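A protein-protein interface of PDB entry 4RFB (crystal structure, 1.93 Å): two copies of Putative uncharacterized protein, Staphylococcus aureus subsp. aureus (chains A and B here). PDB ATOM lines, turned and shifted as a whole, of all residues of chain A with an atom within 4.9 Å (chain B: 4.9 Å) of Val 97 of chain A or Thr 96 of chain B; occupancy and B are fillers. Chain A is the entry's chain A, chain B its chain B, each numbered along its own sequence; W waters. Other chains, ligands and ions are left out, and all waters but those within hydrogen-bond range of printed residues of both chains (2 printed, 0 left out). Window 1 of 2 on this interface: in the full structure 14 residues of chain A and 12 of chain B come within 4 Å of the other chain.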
ATOM      1  N   PHE A  67      -6.660  29.878 -18.459  1.00  0.00           N
ATOM      2  CA  PHE A  67      -5.486  30.600 -18.006  1.00  0.00           C
ATOM      3  C   PHE A  67      -4.495  30.448 -19.181  1.00  0.00           C
ATOM      4  O   PHE A  67      -4.243  29.307 -19.695  1.00  0.00           O
ATOM      5  CB  PHE A  67      -4.907  30.064 -16.679  1.00  0.00           C
ATOM      6  CG  PHE A  67      -3.781  30.910 -16.133  1.00  0.00           C
ATOM      7  CD1 PHE A  67      -4.045  32.146 -15.576  1.00  0.00           C
ATOM      8  CD2 PHE A  67      -2.476  30.486 -16.201  1.00  0.00           C
ATOM      9  CE1 PHE A  67      -3.024  32.955 -15.095  1.00  0.00           C
ATOM     10  CE2 PHE A  67      -1.446  31.281 -15.725  1.00  0.00           C
ATOM     11  CZ  PHE A  67      -1.717  32.503 -15.153  1.00  0.00           C
ATOM     12  N   GLU A  95      -1.435  20.022 -18.923  1.00  0.00           N
ATOM     13  CA  GLU A  95      -1.489  20.463 -17.555  1.00  0.00           C
ATOM     14  C   GLU A  95      -2.617  21.420 -17.224  1.00  0.00           C
ATOM     15  O   GLU A  95      -2.937  22.296 -18.036  1.00  0.00           O
ATOM     16  CB  GLU A  95      -0.195  21.219 -17.195  1.00  0.00           C
ATOM     17  CG  GLU A  95       1.106  20.440 -17.238  1.00  0.00           C
ATOM     18  CD  GLU A  95       1.603  20.152 -18.651  1.00  0.00           C
ATOM     19  OE1 GLU A  95       2.515  19.315 -18.764  1.00  0.00           O
ATOM     20  OE2 GLU A  95       1.078  20.741 -19.637  1.00  0.00           O
ATOM     21  N   THR A  96      -3.247  21.252 -16.055  1.00  0.00           N
ATOM     22  CA  THR A  96      -4.177  22.280 -15.588  1.00  0.00           C
ATOM     23  C   THR A  96      -3.300  23.323 -14.892  1.00  0.00           C
ATOM     24  O   THR A  96      -2.285  22.982 -14.260  1.00  0.00           O
ATOM     25  CB  THR A  96      -5.235  21.803 -14.576  1.00  0.00           C
ATOM     26  OG1 THR A  96      -4.591  21.298 -13.403  1.00  0.00           O
ATOM     27  CG2 THR A  96      -6.133  20.738 -15.175  1.00  0.00           C
ATOM     28  N   VAL A  97      -3.670  24.590 -15.024  1.00  0.00           N
ATOM     29  CA  VAL A  97      -2.933  25.680 -14.355  1.00  0.00           C
ATOM     30  C   VAL A  97      -3.929  26.616 -13.667  1.00  0.00           C
ATOM     31  O   VAL A  97      -4.939  27.047 -14.274  1.00  0.00           O
ATOM     32  CB  VAL A  97      -1.998  26.423 -15.317  1.00  0.00           C
ATOM     33  CG1 VAL A  97      -1.274  27.546 -14.572  1.00  0.00           C
ATOM     34  CG2 VAL A  97      -1.007  25.430 -15.916  1.00  0.00           C
ATOM     35  N   ASN A  98      -3.679  26.873 -12.385  1.00  0.00           N
ATOM     36  CA  ASN A  98      -4.563  27.692 -11.581  1.00  0.00           C
ATOM     37  C   ASN A  98      -5.977  27.152 -11.658  1.00  0.00           C
ATOM     38  O   ASN A  98      -6.958  27.898 -11.708  1.00  0.00           O
ATOM     39  CB  ASN A  98      -4.483  29.175 -11.979  1.00  0.00           C
ATOM     40  CG  ASN A  98      -3.196  29.837 -11.530  1.00  0.00           C
ATOM     41  OD1 ASN A  98      -2.522  29.368 -10.623  1.00  0.00           O
ATOM     42  ND2 ASN A  98      -2.875  30.968 -12.143  1.00  0.00           N
ATOM     43  N   GLY A  99      -6.077  25.830 -11.692  1.00  0.00           N
ATOM     44  CA  GLY A  99      -7.376  25.179 -11.689  1.00  0.00           C
ATOM     45  C   GLY A  99      -8.168  25.328 -12.967  1.00  0.00           C
ATOM     46  O   GLY A  99      -9.355  25.003 -12.993  1.00  0.00           O
ATOM     47  N   ARG A 100      -7.516  25.801 -14.033  1.00  0.00           N
ATOM     48  CA  ARG A 100      -8.168  26.037 -15.329  1.00  0.00           C
ATOM     49  C   ARG A 100      -7.480  25.326 -16.467  1.00  0.00           C
ATOM     50  O   ARG A 100      -6.363  24.869 -16.327  1.00  0.00           O
ATOM     51  CB  ARG A 100      -8.154  27.535 -15.640  1.00  0.00           C
ATOM     52  CG  ARG A 100      -8.910  28.294 -14.577  1.00  0.00           C
ATOM     53  CD  ARG A 100      -8.854  29.774 -14.718  1.00  0.00           C
ATOM     54  NE  ARG A 100      -9.843  30.437 -13.861  1.00  0.00           N
ATOM     55  CZ  ARG A 100      -9.746  30.616 -12.548  1.00  0.00           C
ATOM     56  NH1 ARG A 100      -8.729  30.135 -11.835  1.00  0.00           N
ATOM     57  NH2 ARG A 100     -10.716  31.260 -11.923  1.00  0.00           N
ATOM     58  N   TYR A 102      -5.439  25.216 -19.707  1.00  0.00           N
ATOM     59  CA  TYR A 102      -4.292  26.042 -19.963  1.00  0.00           C
ATOM     60  C   TYR A 102      -3.847  26.004 -21.409  1.00  0.00           C
ATOM     61  O   TYR A 102      -3.848  24.960 -22.054  1.00  0.00           O
ATOM     62  CB  TYR A 102      -3.150  25.515 -19.088  1.00  0.00           C
ATOM     63  CG  TYR A 102      -1.816  26.270 -19.129  1.00  0.00           C
ATOM     64  CD1 TYR A 102      -1.719  27.571 -18.698  1.00  0.00           C
ATOM     65  CD2 TYR A 102      -0.635  25.615 -19.465  1.00  0.00           C
ATOM     66  CE1 TYR A 102      -0.497  28.234 -18.661  1.00  0.00           C
ATOM     67  CE2 TYR A 102       0.595  26.278 -19.447  1.00  0.00           C
ATOM     68  CZ  TYR A 102       0.650  27.592 -19.047  1.00  0.00           C
ATOM     69  OH  TYR A 102       1.858  28.250 -19.007  1.00  0.00           O
ATOM     70  N   GLU B  94       3.749  31.584  -8.294  1.00  0.00           N
ATOM     71  CA  GLU B  94       2.360  31.985  -8.043  1.00  0.00           C
ATOM     72  C   GLU B  94       1.316  31.026  -8.645  1.00  0.00           C
ATOM     73  O   GLU B  94       0.199  30.910  -8.129  1.00  0.00           O
ATOM     74  CB  GLU B  94       2.113  33.409  -8.538  1.00  0.00           C
ATOM     75  CG  GLU B  94       2.630  34.448  -7.562  1.00  0.00           C
ATOM     76  CD  GLU B  94       4.111  34.347  -7.323  1.00  0.00           C
ATOM     77  OE1 GLU B  94       4.884  34.398  -8.317  1.00  0.00           O
ATOM     78  OE2 GLU B  94       4.507  34.252  -6.125  1.00  0.00           O
ATOM     79  N   GLU B  95       1.695  30.338  -9.715  1.00  0.00           N
ATOM     80  CA  GLU B  95       0.799  29.416 -10.371  1.00  0.00           C
ATOM     81  C   GLU B  95       0.775  28.062  -9.696  1.00  0.00           C
ATOM     82  O   GLU B  95       1.796  27.596  -9.217  1.00  0.00           O
ATOM     83  CB  GLU B  95       1.217  29.186 -11.838  1.00  0.00           C
ATOM     84  CG  GLU B  95       1.059  30.353 -12.790  1.00  0.00           C
ATOM     85  CD  GLU B  95       2.001  31.528 -12.538  1.00  0.00           C
ATOM     86  OE1 GLU B  95       1.511  32.674 -12.677  1.00  0.00           O
ATOM     87  OE2 GLU B  95       3.208  31.306 -12.231  1.00  0.00           O
ATOM     88  N   THR B  96      -0.409  27.453  -9.617  1.00  0.00           N
ATOM     89  CA  THR B  96      -0.488  26.050  -9.250  1.00  0.00           C
ATOM     90  C   THR B  96      -0.563  25.320 -10.593  1.00  0.00           C
ATOM     91  O   THR B  96      -1.133  25.842 -11.569  1.00  0.00           O
ATOM     92  CB  THR B  96      -1.723  25.723  -8.411  1.00  0.00           C
ATOM     93  OG1 THR B  96      -2.901  26.099  -9.121  1.00  0.00           O
ATOM     94  CG2 THR B  96      -1.686  26.473  -7.102  1.00  0.00           C
ATOM     95  N   VAL B  97       0.010  24.129 -10.650  1.00  0.00           N
ATOM     96  CA  VAL B  97       0.027  23.314 -11.852  1.00  0.00           C
ATOM     97  C   VAL B  97      -0.420  21.916 -11.457  1.00  0.00           C
ATOM     98  O   VAL B  97       0.150  21.302 -10.536  1.00  0.00           O
ATOM     99  CB  VAL B  97       1.437  23.288 -12.493  1.00  0.00           C
ATOM    100  CG1 VAL B  97       1.429  22.455 -13.770  1.00  0.00           C
ATOM    101  CG2 VAL B  97       1.906  24.707 -12.780  1.00  0.00           C
ATOM    102  N   ASN B  98      -1.462  21.416 -12.111  1.00  0.00           N
ATOM    103  CA  ASN B  98      -2.023  20.092 -11.761  1.00  0.00           C
ATOM    104  C   ASN B  98      -2.324  19.939 -10.298  1.00  0.00           C
ATOM    105  O   ASN B  98      -2.096  18.874  -9.705  1.00  0.00           O
ATOM    106  CB  ASN B  98      -1.117  18.960 -12.268  1.00  0.00           C
ATOM    107  CG  ASN B  98      -1.161  18.839 -13.771  1.00  0.00           C
ATOM    108  OD1 ASN B  98      -2.162  19.203 -14.388  1.00  0.00           O
ATOM    109  ND2 ASN B  98      -0.090  18.333 -14.369  1.00  0.00           N
ATOM    110  N   GLY B  99      -2.846  21.012  -9.712  1.00  0.00           N
ATOM    111  CA  GLY B  99      -3.210  21.026  -8.321  1.00  0.00           C
ATOM    112  C   GLY B  99      -2.061  21.004  -7.330  1.00  0.00           C
ATOM    113  O   GLY B  99      -2.285  20.785  -6.150  1.00  0.00           O
ATOM    114  N   ARG B 100      -0.844  21.266  -7.789  1.00  0.00           N
ATOM    115  CA  ARG B 100       0.329  21.247  -6.930  1.00  0.00           C
ATOM    116  C   ARG B 100       1.085  22.554  -6.959  1.00  0.00           C
ATOM    117  O   ARG B 100       0.974  23.339  -7.908  1.00  0.00           O
ATOM    118  CB  ARG B 100       1.283  20.147  -7.429  1.00  0.00           C
ATOM    119  CG  ARG B 100       0.654  18.760  -7.309  1.00  0.00           C
ATOM    120  CD  ARG B 100       1.295  17.762  -8.232  1.00  0.00           C
ATOM    121  NE  ARG B 100       0.897  16.401  -7.887  1.00  0.00           N
ATOM    122  CZ  ARG B 100      -0.218  15.775  -8.253  1.00  0.00           C
ATOM    123  NH1 ARG B 100      -1.136  16.337  -9.040  1.00  0.00           N
ATOM    124  NH2 ARG B 100      -0.396  14.524  -7.834  1.00  0.00           N
ATOM    125  N   TYR B 102       4.192  24.842  -7.575  1.00  0.00           N
ATOM    126  CA  TYR B 102       5.031  24.828  -8.744  1.00  0.00           C
ATOM    127  C   TYR B 102       6.346  25.586  -8.536  1.00  0.00           C
ATOM    128  O   TYR B 102       6.388  26.603  -7.841  1.00  0.00           O
ATOM    129  CB  TYR B 102       4.224  25.491  -9.876  1.00  0.00           C
ATOM    130  CG  TYR B 102       4.887  25.580 -11.264  1.00  0.00           C
ATOM    131  CD1 TYR B 102       5.233  24.432 -11.960  1.00  0.00           C
ATOM    132  CD2 TYR B 102       5.052  26.804 -11.914  1.00  0.00           C
ATOM    133  CE1 TYR B 102       5.803  24.494 -13.227  1.00  0.00           C
ATOM    134  CE2 TYR B 102       5.622  26.881 -13.209  1.00  0.00           C
ATOM    135  CZ  TYR B 102       5.992  25.706 -13.850  1.00  0.00           C
ATOM    136  OH  TYR B 102       6.525  25.716 -15.133  1.00  0.00           O
HETATM  137  O   HOH W   1      -0.725  32.753 -11.245  1.00  0.00           O
HETATM  138  O   HOH W   2      -2.591  30.189  -7.938  1.00  0.00           O
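Glu 95 of chain A touches Val 97 of chain B, but with the chains exchanged Val 97 of chain A does not touch Glu 95 of chain B (4.05 Å).
Glu 95 of chain A touches Asn 98 of chain B, and with the chains exchanged Asn 98 of chain A touches Glu 95 of chain B.
Thr 96 of chain A touches Val 97 of chain B, and with the chains exchanged Val 97 of chain A touches Thr 96 of chain B.
Thr 96 of chain A touches Asn 98 of chain B, and with the chains exchanged Asn 98 of chain A touches Thr 96 of chain B.
Positions printed for both chains: 95, 96, 97, 98, 99, 100 and 102.
Of the 8 pairs that touch across the chains among the printed residues, 6 have their exchanged pair printed and touching as well.
The guanidinium group (NH1) of Arg 100 of chain B is in hydrogen-bond range of the backbone carbonyl oxygen (O) of Asn 98 of chain B (2.8 Å).
The guanidinium group (NH1) of Arg 100 of chain A lies within hydrogen-bond range of the backbone carbonyl oxygen (O) of Asn 98 of chain A, at 2.9 Å.
Water W1 lies within hydrogen-bond range of OE1 of Glu 95 of chain B (2.7 Å) and ND2 of Asn 98 of chain A (2.9 Å).
Water W2 lies within hydrogen-bond range of OD1 of Asn 98 of chain A and O of Glu 94 of chain B.
Of the 8 printed residues of chain B, 4 touch a printed residue of chain A.
Hydrophobic or aromatic side chains of chain B that line the printed part of chain A: Val 97.
Of the 8 printed residues of chain A, 5 touch a printed residue of chain B.
Printed residues of chain A that touch a printed residue of chain B: Phe 67, Glu 95, Thr 96, Val 97 and Asn 98.
Hydrophobic or aromatic side chains of chain A that line the printed part of chain B: Phe 67 and Val 97.
Among the printed residues, 8 pairs touch across the chains.
Among the printed residues, no Asp or Glu carboxylate lies within 4 Å of a Lys or Arg side-chain nitrogen of the other chain.
N of Asn 98 of chain B lies within hydrogen-bond range of O of Thr 96 of chain A (2.8 Å).
The backbone carbonyl oxygen (O) of Thr 96 of chain B is in hydrogen-bond range of the backbone NH (N) of Asn 98 of chain A, at 2.9 Å.
Of chain B, only Thr 96 comes within 4 Å of Val 97 of chain A.
Printed residues of chain A within 4 Å of Thr 96 of chain B: Val 97 (3.3 Å) and Asn 98 (2.9 Å).
Printed residues of chain B within 4 Å of Thr 96 of chain A: Val 97 and Asn 98.
Printed residues of chain A within 4 Å of Glu 95 of chain B: Phe 67 and Asn 98.
Printed residues of chain B within 4 Å of Glu 95 of chain A: Val 97 and Asn 98.
Arg 100 of chain B touches none of the printed residues of chain A.
Gly 99 of chain B touches none of the printed residues of chain A.
The nearest residue of chain B that does not touch Val 97 of chain A is Glu 95 of chain B (4.05 Å).
Glu 95 of chain B touches Phe 67 of chain A (CG to CE2, 3.97 Å).
Val 97 of chain B touches Glu 95 of chain A.
Glu 95 of chain A touches Asn 98 of chain B (CA to OD1, 3.5 Å).
Val 97 of chain B touches Thr 96 of chain A.
Val 97 of chain A touches Thr 96 of chain B (CA to O, 3.3 Å).
Glu 95 of chain B touches Asn 98 of chain A.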
